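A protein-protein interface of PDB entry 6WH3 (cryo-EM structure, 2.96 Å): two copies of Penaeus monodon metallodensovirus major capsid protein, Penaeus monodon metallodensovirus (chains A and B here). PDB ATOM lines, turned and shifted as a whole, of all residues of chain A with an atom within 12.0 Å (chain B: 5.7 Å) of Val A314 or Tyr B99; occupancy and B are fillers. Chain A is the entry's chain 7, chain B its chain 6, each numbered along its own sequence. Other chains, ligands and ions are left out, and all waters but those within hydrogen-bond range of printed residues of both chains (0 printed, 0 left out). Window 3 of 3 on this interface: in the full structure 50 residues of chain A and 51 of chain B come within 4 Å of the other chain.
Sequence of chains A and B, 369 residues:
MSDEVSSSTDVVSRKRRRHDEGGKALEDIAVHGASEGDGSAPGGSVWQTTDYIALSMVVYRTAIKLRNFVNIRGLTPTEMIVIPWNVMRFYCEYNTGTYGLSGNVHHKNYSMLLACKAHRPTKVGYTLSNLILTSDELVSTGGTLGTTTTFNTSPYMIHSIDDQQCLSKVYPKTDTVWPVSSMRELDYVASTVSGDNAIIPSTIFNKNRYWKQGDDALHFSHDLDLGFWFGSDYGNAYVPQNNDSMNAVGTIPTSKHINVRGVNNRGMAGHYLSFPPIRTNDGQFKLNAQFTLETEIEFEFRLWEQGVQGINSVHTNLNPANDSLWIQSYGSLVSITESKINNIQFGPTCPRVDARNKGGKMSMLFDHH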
ATOM      1  N   TYR A  52      -5.260 -28.298   6.359  1.00  0.00           N
ATOM      2  CA  TYR A  52      -6.221 -27.267   6.007  1.00  0.00           C
ATOM      3  C   TYR A  52      -6.425 -27.087   4.510  1.00  0.00           C
ATOM      4  O   TYR A  52      -7.304 -26.317   4.119  1.00  0.00           O
ATOM      5  CB  TYR A  52      -5.823 -25.921   6.604  1.00  0.00           C
ATOM      6  CG  TYR A  52      -5.966 -25.838   8.094  1.00  0.00           C
ATOM      7  CD1 TYR A  52      -6.991 -26.497   8.739  1.00  0.00           C
ATOM      8  CD2 TYR A  52      -5.152 -25.012   8.840  1.00  0.00           C
ATOM      9  CE1 TYR A  52      -7.155 -26.400  10.088  1.00  0.00           C
ATOM     10  CE2 TYR A  52      -5.314 -24.901  10.192  1.00  0.00           C
ATOM     11  CZ  TYR A  52      -6.320 -25.596  10.809  1.00  0.00           C
ATOM     12  OH  TYR A  52      -6.490 -25.493  12.163  1.00  0.00           O
ATOM     13  N   LYS A 117     -15.424 -17.485  -1.694  1.00  0.00           N
ATOM     14  CA  LYS A 117     -14.292 -16.676  -2.125  1.00  0.00           C
ATOM     15  C   LYS A 117     -14.019 -16.775  -3.613  1.00  0.00           C
ATOM     16  O   LYS A 117     -13.426 -15.852  -4.179  1.00  0.00           O
ATOM     17  CB  LYS A 117     -13.013 -17.048  -1.388  1.00  0.00           C
ATOM     18  CG  LYS A 117     -12.440 -18.395  -1.688  1.00  0.00           C
ATOM     19  CD  LYS A 117     -11.140 -18.470  -0.938  1.00  0.00           C
ATOM     20  CE  LYS A 117     -10.195 -17.414  -1.480  1.00  0.00           C
ATOM     21  NZ  LYS A 117      -8.901 -17.363  -0.770  1.00  0.00           N
ATOM     22  N   TRP A 304     -13.757 -20.751   1.761  1.00  0.00           N
ATOM     23  CA  TRP A 304     -12.710 -20.008   2.437  1.00  0.00           C
ATOM     24  C   TRP A 304     -11.683 -20.935   3.078  1.00  0.00           C
ATOM     25  O   TRP A 304     -11.924 -22.122   3.297  1.00  0.00           O
ATOM     26  CB  TRP A 304     -13.333 -19.089   3.472  1.00  0.00           C
ATOM     27  CG  TRP A 304     -14.218 -18.100   2.829  1.00  0.00           C
ATOM     28  CD1 TRP A 304     -15.562 -18.196   2.677  1.00  0.00           C
ATOM     29  CD2 TRP A 304     -13.829 -16.879   2.203  1.00  0.00           C
ATOM     30  NE1 TRP A 304     -16.042 -17.100   2.018  1.00  0.00           N
ATOM     31  CE2 TRP A 304     -14.994 -16.274   1.715  1.00  0.00           C
ATOM     32  CE3 TRP A 304     -12.610 -16.233   2.019  1.00  0.00           C
ATOM     33  CZ2 TRP A 304     -14.977 -15.059   1.054  1.00  0.00           C
ATOM     34  CZ3 TRP A 304     -12.596 -15.029   1.366  1.00  0.00           C
ATOM     35  CH2 TRP A 304     -13.770 -14.453   0.890  1.00  0.00           C
ATOM     36  N   GLU A 305     -10.516 -20.367   3.365  1.00  0.00           N
ATOM     37  CA  GLU A 305      -9.422 -21.121   3.957  1.00  0.00           C
ATOM     38  C   GLU A 305      -9.790 -21.611   5.349  1.00  0.00           C
ATOM     39  O   GLU A 305     -10.391 -20.887   6.142  1.00  0.00           O
ATOM     40  CB  GLU A 305      -8.176 -20.248   4.044  1.00  0.00           C
ATOM     41  CG  GLU A 305      -7.684 -19.751   2.720  1.00  0.00           C
ATOM     42  CD  GLU A 305      -8.385 -18.485   2.306  1.00  0.00           C
ATOM     43  OE1 GLU A 305      -9.272 -18.034   3.055  1.00  0.00           O
ATOM     44  OE2 GLU A 305      -8.065 -17.943   1.232  1.00  0.00           O
ATOM     45  N   GLN A 306      -9.414 -22.848   5.649  1.00  0.00           N
ATOM     46  CA  GLN A 306      -9.633 -23.385   6.978  1.00  0.00           C
ATOM     47  C   GLN A 306      -8.639 -22.799   7.969  1.00  0.00           C
ATOM     48  O   GLN A 306      -7.571 -22.308   7.604  1.00  0.00           O
ATOM     49  CB  GLN A 306      -9.509 -24.901   6.984  1.00  0.00           C
ATOM     50  CG  GLN A 306     -10.568 -25.599   6.211  1.00  0.00           C
ATOM     51  CD  GLN A 306     -11.936 -25.265   6.716  1.00  0.00           C
ATOM     52  OE1 GLN A 306     -12.143 -25.108   7.911  1.00  0.00           O
ATOM     53  NE2 GLN A 306     -12.888 -25.173   5.810  1.00  0.00           N
ATOM     54  N   GLY A 307      -9.002 -22.866   9.234  1.00  0.00           N
ATOM     55  CA  GLY A 307      -8.121 -22.423  10.282  1.00  0.00           C
ATOM     56  C   GLY A 307      -8.357 -20.982  10.656  1.00  0.00           C
ATOM     57  O   GLY A 307      -9.322 -20.338  10.243  1.00  0.00           O
ATOM     58  N   VAL A 308      -7.439 -20.469  11.474  1.00  0.00           N
ATOM     59  CA  VAL A 308      -7.498 -19.072  11.873  1.00  0.00           C
ATOM     60  C   VAL A 308      -7.376 -18.164  10.665  1.00  0.00           C
ATOM     61  O   VAL A 308      -7.852 -17.029  10.693  1.00  0.00           O
ATOM     62  CB  VAL A 308      -6.404 -18.788  12.918  1.00  0.00           C
ATOM     63  CG1 VAL A 308      -6.396 -17.334  13.316  1.00  0.00           C
ATOM     64  CG2 VAL A 308      -6.612 -19.660  14.123  1.00  0.00           C
ATOM     65  N   GLN A 309      -6.778 -18.654   9.582  1.00  0.00           N
ATOM     66  CA  GLN A 309      -6.677 -17.854   8.369  1.00  0.00           C
ATOM     67  C   GLN A 309      -8.046 -17.443   7.850  1.00  0.00           C
ATOM     68  O   GLN A 309      -8.187 -16.373   7.254  1.00  0.00           O
ATOM     69  CB  GLN A 309      -5.936 -18.634   7.296  1.00  0.00           C
ATOM     70  CG  GLN A 309      -5.597 -17.813   6.092  1.00  0.00           C
ATOM     71  CD  GLN A 309      -4.800 -18.590   5.091  1.00  0.00           C
ATOM     72  OE1 GLN A 309      -4.487 -19.756   5.303  1.00  0.00           O
ATOM     73  NE2 GLN A 309      -4.431 -17.944   4.010  1.00  0.00           N
ATOM     74  N   GLY A 310      -9.060 -18.270   8.069  1.00  0.00           N
ATOM     75  CA  GLY A 310     -10.402 -18.008   7.606  1.00  0.00           C
ATOM     76  C   GLY A 310     -11.289 -17.258   8.568  1.00  0.00           C
ATOM     77  O   GLY A 310     -12.482 -17.109   8.299  1.00  0.00           O
ATOM     78  N   ILE A 311     -10.755 -16.785   9.691  1.00  0.00           N
ATOM     79  CA  ILE A 311     -11.535 -15.981  10.619  1.00  0.00           C
ATOM     80  C   ILE A 311     -11.767 -14.602  10.025  1.00  0.00           C
ATOM     81  O   ILE A 311     -10.842 -13.977   9.496  1.00  0.00           O
ATOM     82  CB  ILE A 311     -10.811 -15.897  11.969  1.00  0.00           C
ATOM     83  CG1 ILE A 311     -10.634 -17.288  12.566  1.00  0.00           C
ATOM     84  CG2 ILE A 311     -11.523 -14.974  12.908  1.00  0.00           C
ATOM     85  CD1 ILE A 311     -11.913 -18.014  12.782  1.00  0.00           C
ATOM     86  N   ASN A 312     -13.007 -14.111  10.121  1.00  0.00           N
ATOM     87  CA  ASN A 312     -13.365 -12.841   9.492  1.00  0.00           C
ATOM     88  C   ASN A 312     -12.426 -11.716   9.900  1.00  0.00           C
ATOM     89  O   ASN A 312     -11.962 -10.944   9.055  1.00  0.00           O
ATOM     90  CB  ASN A 312     -14.802 -12.464   9.838  1.00  0.00           C
ATOM     91  CG  ASN A 312     -15.818 -13.294   9.102  1.00  0.00           C
ATOM     92  OD1 ASN A 312     -16.077 -13.067   7.924  1.00  0.00           O
ATOM     93  ND2 ASN A 312     -16.413 -14.249   9.791  1.00  0.00           N
ATOM     94  N   SER A 313     -12.144 -11.598  11.194  1.00  0.00           N
ATOM     95  CA  SER A 313     -11.371 -10.453  11.663  1.00  0.00           C
ATOM     96  C   SER A 313      -9.950 -10.481  11.124  1.00  0.00           C
ATOM     97  O   SER A 313      -9.413  -9.442  10.726  1.00  0.00           O
ATOM     98  CB  SER A 313     -11.363 -10.410  13.188  1.00  0.00           C
ATOM     99  OG  SER A 313     -10.696 -11.536  13.723  1.00  0.00           O
ATOM    100  N   VAL A 314      -9.315 -11.653  11.112  1.00  0.00           N
ATOM    101  CA  VAL A 314      -7.930 -11.759  10.674  1.00  0.00           C
ATOM    102  C   VAL A 314      -7.799 -12.174   9.219  1.00  0.00           C
ATOM    103  O   VAL A 314      -6.677 -12.234   8.710  1.00  0.00           O
ATOM    104  CB  VAL A 314      -7.140 -12.734  11.565  1.00  0.00           C
ATOM    105  CG1 VAL A 314      -7.100 -12.228  12.989  1.00  0.00           C
ATOM    106  CG2 VAL A 314      -7.750 -14.091  11.509  1.00  0.00           C
ATOM    107  N   HIS A 315      -8.900 -12.455   8.528  1.00  0.00           N
ATOM    108  CA  HIS A 315      -8.778 -12.860   7.134  1.00  0.00           C
ATOM    109  C   HIS A 315      -8.417 -11.703   6.222  1.00  0.00           C
ATOM    110  O   HIS A 315      -7.901 -11.936   5.126  1.00  0.00           O
ATOM    111  CB  HIS A 315     -10.064 -13.504   6.635  1.00  0.00           C
ATOM    112  CG  HIS A 315      -9.960 -14.052   5.250  1.00  0.00           C
ATOM    113  ND1 HIS A 315     -10.103 -13.266   4.128  1.00  0.00           N
ATOM    114  CD2 HIS A 315      -9.713 -15.305   4.802  1.00  0.00           C
ATOM    115  CE1 HIS A 315      -9.955 -14.013   3.049  1.00  0.00           C
ATOM    116  NE2 HIS A 315      -9.719 -15.254   3.431  1.00  0.00           N
ATOM    117  N   THR A 316      -8.681 -10.467   6.637  1.00  0.00           N
ATOM    118  CA  THR A 316      -8.330  -9.331   5.798  1.00  0.00           C
ATOM    119  C   THR A 316      -6.833  -9.300   5.532  1.00  0.00           C
ATOM    120  O   THR A 316      -6.393  -9.265   4.379  1.00  0.00           O
ATOM    121  CB  THR A 316      -8.787  -8.034   6.458  1.00  0.00           C
ATOM    122  OG1 THR A 316      -8.151  -7.900   7.731  1.00  0.00           O
ATOM    123  CG2 THR A 316     -10.288  -8.055   6.658  1.00  0.00           C
ATOM    124  N   ASN A 317      -6.034  -9.312   6.593  1.00  0.00           N
ATOM    125  CA  ASN A 317      -4.588  -9.248   6.472  1.00  0.00           C
ATOM    126  C   ASN A 317      -3.900 -10.608   6.431  1.00  0.00           C
ATOM    127  O   ASN A 317      -2.700 -10.659   6.149  1.00  0.00           O
ATOM    128  CB  ASN A 317      -4.035  -8.392   7.613  1.00  0.00           C
ATOM    129  CG  ASN A 317      -4.459  -8.895   8.965  1.00  0.00           C
ATOM    130  OD1 ASN A 317      -5.352  -9.730   9.070  1.00  0.00           O
ATOM    131  ND2 ASN A 317      -3.847  -8.365  10.013  1.00  0.00           N
ATOM    132  N   LEU A 318      -4.600 -11.705   6.701  1.00  0.00           N
ATOM    133  CA  LEU A 318      -4.073 -13.038   6.427  1.00  0.00           C
ATOM    134  C   LEU A 318      -4.554 -13.628   5.112  1.00  0.00           C
ATOM    135  O   LEU A 318      -4.252 -14.787   4.830  1.00  0.00           O
ATOM    136  CB  LEU A 318      -4.396 -14.006   7.564  1.00  0.00           C
ATOM    137  CG  LEU A 318      -3.353 -14.108   8.672  1.00  0.00           C
ATOM    138  CD1 LEU A 318      -3.196 -12.810   9.429  1.00  0.00           C
ATOM    139  CD2 LEU A 318      -3.754 -15.207   9.602  1.00  0.00           C
ATOM    140  N   ASN A 319      -5.321 -12.885   4.332  1.00  0.00           N
ATOM    141  CA  ASN A 319      -5.714 -13.351   3.014  1.00  0.00           C
ATOM    142  C   ASN A 319      -4.465 -13.673   2.200  1.00  0.00           C
ATOM    143  O   ASN A 319      -3.516 -12.879   2.199  1.00  0.00           O
ATOM    144  CB  ASN A 319      -6.541 -12.285   2.304  1.00  0.00           C
ATOM    145  CG  ASN A 319      -7.253 -12.811   1.089  1.00  0.00           C
ATOM    146  OD1 ASN A 319      -7.659 -13.966   1.048  1.00  0.00           O
ATOM    147  ND2 ASN A 319      -7.395 -11.969   0.079  1.00  0.00           N
ATOM    148  N   PRO A 320      -4.413 -14.816   1.521  1.00  0.00           N
ATOM    149  CA  PRO A 320      -3.224 -15.141   0.729  1.00  0.00           C
ATOM    150  C   PRO A 320      -3.011 -14.125  -0.377  1.00  0.00           C
ATOM    151  O   PRO A 320      -3.949 -13.731  -1.070  1.00  0.00           O
ATOM    152  CB  PRO A 320      -3.548 -16.518   0.152  1.00  0.00           C
ATOM    153  CG  PRO A 320      -4.524 -17.080   1.060  1.00  0.00           C
ATOM    154  CD  PRO A 320      -5.357 -15.940   1.546  1.00  0.00           C
ATOM    155  N   ALA A 321      -1.766 -13.697  -0.542  1.00  0.00           N
ATOM    156  CA  ALA A 321      -1.454 -12.833  -1.667  1.00  0.00           C
ATOM    157  C   ALA A 321      -1.409 -13.592  -2.978  1.00  0.00           C
ATOM    158  O   ALA A 321      -1.369 -12.961  -4.037  1.00  0.00           O
ATOM    159  CB  ALA A 321      -0.124 -12.123  -1.443  1.00  0.00           C
ATOM    160  N   ASP A 323      -3.878 -15.454  -3.953  1.00  0.00           N
ATOM    161  CA  ASP A 323      -5.198 -15.428  -4.568  1.00  0.00           C
ATOM    162  C   ASP A 323      -5.107 -14.873  -5.975  1.00  0.00           C
ATOM    163  O   ASP A 323      -5.628 -15.463  -6.923  1.00  0.00           O
ATOM    164  CB  ASP A 323      -6.170 -14.599  -3.737  1.00  0.00           C
ATOM    165  CG  ASP A 323      -6.578 -15.288  -2.471  1.00  0.00           C
ATOM    166  OD1 ASP A 323      -6.328 -16.501  -2.349  1.00  0.00           O
ATOM    167  OD2 ASP A 323      -7.182 -14.622  -1.611  1.00  0.00           O
ATOM    168  N   TYR B  94     -13.820 -18.435  16.921  1.00  0.00           N
ATOM    169  CA  TYR B  94     -12.508 -18.665  17.499  1.00  0.00           C
ATOM    170  C   TYR B  94     -12.354 -17.685  18.648  1.00  0.00           C
ATOM    171  O   TYR B  94     -12.052 -16.514  18.439  1.00  0.00           O
ATOM    172  CB  TYR B  94     -11.455 -18.459  16.418  1.00  0.00           C
ATOM    173  CG  TYR B  94     -10.026 -18.718  16.800  1.00  0.00           C
ATOM    174  CD1 TYR B  94      -9.546 -20.009  16.882  1.00  0.00           C
ATOM    175  CD2 TYR B  94      -9.148 -17.680  17.025  1.00  0.00           C
ATOM    176  CE1 TYR B  94      -8.248 -20.260  17.207  1.00  0.00           C
ATOM    177  CE2 TYR B  94      -7.840 -17.925  17.353  1.00  0.00           C
ATOM    178  CZ  TYR B  94      -7.399 -19.220  17.442  1.00  0.00           C
ATOM    179  OH  TYR B  94      -6.094 -19.482  17.766  1.00  0.00           O
ATOM    180  N   ASN B  95     -12.467 -18.169  19.871  1.00  0.00           N
ATOM    181  CA  ASN B  95     -12.356 -17.283  21.017  1.00  0.00           C
ATOM    182  C   ASN B  95     -11.084 -17.679  21.740  1.00  0.00           C
ATOM    183  O   ASN B  95     -11.053 -18.668  22.471  1.00  0.00           O
ATOM    184  CB  ASN B  95     -13.581 -17.416  21.911  1.00  0.00           C
ATOM    185  CG  ASN B  95     -14.853 -16.972  21.229  1.00  0.00           C
ATOM    186  OD1 ASN B  95     -15.850 -17.689  21.225  1.00  0.00           O
ATOM    187  ND2 ASN B  95     -14.838 -15.773  20.674  1.00  0.00           N
ATOM    188  N   THR B  96     -10.046 -16.874  21.562  1.00  0.00           N
ATOM    189  CA  THR B  96      -8.779 -17.083  22.237  1.00  0.00           C
ATOM    190  C   THR B  96      -8.176 -15.721  22.511  1.00  0.00           C
ATOM    191  O   THR B  96      -8.100 -14.901  21.594  1.00  0.00           O
ATOM    192  CB  THR B  96      -7.841 -17.931  21.382  1.00  0.00           C
ATOM    193  OG1 THR B  96      -8.446 -19.203  21.138  1.00  0.00           O
ATOM    194  CG2 THR B  96      -6.520 -18.139  22.093  1.00  0.00           C
ATOM    195  N   GLY B  97      -7.741 -15.483  23.739  1.00  0.00           N
ATOM    196  CA  GLY B  97      -6.966 -14.290  24.000  1.00  0.00           C
ATOM    197  C   GLY B  97      -7.649 -13.020  23.543  1.00  0.00           C
ATOM    198  O   GLY B  97      -8.785 -12.733  23.928  1.00  0.00           O
ATOM    199  N   THR B  98      -6.957 -12.261  22.696  1.00  0.00           N
ATOM    200  CA  THR B  98      -7.458 -10.986  22.208  1.00  0.00           C
ATOM    201  C   THR B  98      -8.509 -11.142  21.113  1.00  0.00           C
ATOM    202  O   THR B  98      -9.307 -10.220  20.909  1.00  0.00           O
ATOM    203  CB  THR B  98      -6.277 -10.149  21.707  1.00  0.00           C
ATOM    204  OG1 THR B  98      -5.348  -9.961  22.781  1.00  0.00           O
ATOM    205  CG2 THR B  98      -6.726  -8.780  21.220  1.00  0.00           C
ATOM    206  N   TYR B  99      -8.551 -12.288  20.429  1.00  0.00           N
ATOM    207  CA  TYR B  99      -9.489 -12.467  19.323  1.00  0.00           C
ATOM    208  C   TYR B  99     -10.922 -12.209  19.762  1.00  0.00           C
ATOM    209  O   TYR B  99     -11.624 -11.379  19.175  1.00  0.00           O
ATOM    210  CB  TYR B  99      -9.367 -13.875  18.750  1.00  0.00           C
ATOM    211  CG  TYR B  99      -8.053 -14.186  18.091  1.00  0.00           C
ATOM    212  CD1 TYR B  99      -7.843 -13.917  16.751  1.00  0.00           C
ATOM    213  CD2 TYR B  99      -7.028 -14.770  18.808  1.00  0.00           C
ATOM    214  CE1 TYR B  99      -6.643 -14.216  16.152  1.00  0.00           C
ATOM    215  CE2 TYR B  99      -5.832 -15.069  18.223  1.00  0.00           C
ATOM    216  CZ  TYR B  99      -5.642 -14.792  16.897  1.00  0.00           C
ATOM    217  OH  TYR B  99      -4.436 -15.106  16.331  1.00  0.00           O
ATOM    218  N   GLY B 100     -11.377 -12.916  20.796  1.00  0.00           N
ATOM    219  CA  GLY B 100     -12.744 -12.762  21.262  1.00  0.00           C
ATOM    220  C   GLY B 100     -13.114 -11.341  21.624  1.00  0.00           C
ATOM    221  O   GLY B 100     -14.298 -10.991  21.599  1.00  0.00           O
ATOM    222  N   LEU B 101     -12.127 -10.513  21.964  1.00  0.00           N
ATOM    223  CA  LEU B 101     -12.398  -9.106  22.226  1.00  0.00           C
ATOM    224  C   LEU B 101     -12.642  -8.347  20.928  1.00  0.00           C
ATOM    225  O   LEU B 101     -13.484  -7.443  20.877  1.00  0.00           O
ATOM    226  CB  LEU B 101     -11.239  -8.481  23.004  1.00  0.00           C
ATOM    227  CG  LEU B 101     -10.909  -8.868  24.454  1.00  0.00           C
ATOM    228  CD1 LEU B 101     -10.787 -10.358  24.697  1.00  0.00           C
ATOM    229  CD2 LEU B 101      -9.626  -8.175  24.878  1.00  0.00           C
ATOM    230  N   SER B 102     -11.914  -8.697  19.873  1.00  0.00           N
ATOM    231  CA  SER B 102     -12.132  -8.096  18.569  1.00  0.00           C
ATOM    232  C   SER B 102     -13.428  -8.618  17.955  1.00  0.00           C
ATOM    233  O   SER B 102     -13.954  -9.667  18.338  1.00  0.00           O
ATOM    234  CB  SER B 102     -10.950  -8.380  17.642  1.00  0.00           C
ATOM    235  OG  SER B 102     -10.813  -9.768  17.399  1.00  0.00           O
ATOM    236  N   GLY B 103     -13.948  -7.867  16.994  1.00  0.00           N
ATOM    237  CA  GLY B 103     -15.257  -8.146  16.445  1.00  0.00           C
ATOM    238  C   GLY B 103     -15.258  -9.162  15.317  1.00  0.00           C
ATOM    239  O   GLY B 103     -14.293  -9.296  14.571  1.00  0.00           O
ATOM    240  N   VAL B 105     -15.378 -12.676  14.904  1.00  0.00           N
ATOM    241  CA  VAL B 105     -14.336 -13.690  14.859  1.00  0.00           C
ATOM    242  C   VAL B 105     -14.857 -15.001  14.278  1.00  0.00           C
ATOM    243  O   VAL B 105     -14.135 -16.005  14.258  1.00  0.00           O
ATOM    244  CB  VAL B 105     -13.742 -13.828  16.275  1.00  0.00           C
ATOM    245  CG1 VAL B 105     -12.565 -14.723  16.268  1.00  0.00           C
ATOM    246  CG2 VAL B 105     -13.346 -12.476  16.795  1.00  0.00           C
ATOM    247  N   SER B 181     -15.855 -14.758  25.157  1.00  0.00           N
ATOM    248  CA  SER B 181     -14.675 -14.417  24.375  1.00  0.00           C
ATOM    249  C   SER B 181     -13.490 -15.302  24.713  1.00  0.00           C
ATOM    250  O   SER B 181     -12.527 -15.353  23.944  1.00  0.00           O
ATOM    251  CB  SER B 181     -14.292 -12.961  24.615  1.00  0.00           C
ATOM    252  OG  SER B 181     -13.909 -12.761  25.962  1.00  0.00           O
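The side-chain amide oxygen (OD1) of Asn A317 sits close to the backbone carbonyl oxygen (O) of Val A314 (2.9 Å).
OG of Ser B102 is in hydrogen-bond range of O of Tyr B99, at 2.5 Å.
Among the printed residues, pairs that only touch across the chains: Val A308 with Tyr B94, Ile A311 with Tyr B94, Ile A311 with Val B105, Ser A313 with Gly B103 and Val A314 with Tyr B99.
Of the printed residues of chain B, Val A308 touches Tyr B94 (3.4 Å).
Of the printed residues of chain B, Ile A311 touches Tyr B94 (3.7 Å) and Val B105 (3.1 Å).
Of the printed residues of chain B, Ser A313 touches Gly B103.
Of the printed residues of chain B, Val A314 touches Tyr B99.
Asn A317 touches none of the printed residues of chain B.
Ala A321 touches none of the printed residues of chain B.
Printed residues of chain A within 4 Å of Tyr B94: Val A308 (3.4 Å) and Ile A311 (3.7 Å).
Thr B98 touches none of the printed residues of chain A.
No residue of chain A comes within 4 Å of Leu B101.
No residue of chain A comes within 4 Å of Ser B102.
Of chain A, only Ser A313 (3.4 Å) comes within 4 Å of Gly B103.
Val B105 touches just one residue of chain A: Ile A311 (3.1 Å).
The nearest residue of chain A that does not touch Tyr B99 is Val A308 (4.2 Å).
Of the 12 printed residues of chain B, 4 touch a printed residue of chain A.
Printed residues of chain A that touch a printed residue of chain B: Val A308, Ile A311, Ser A313 and Val A314.
Along chain A the printed residues that touch a printed residue of chain B span positions 308 to 314.
Among the printed residues, no Asp or Glu carboxylate lies within 4 Å of a Lys or Arg side-chain nitrogen of the other chain.
No position is printed for both chains.
Of the 5 pairs that touch across the chains among the printed residues, none has its exchanged pair printed and touching as well.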
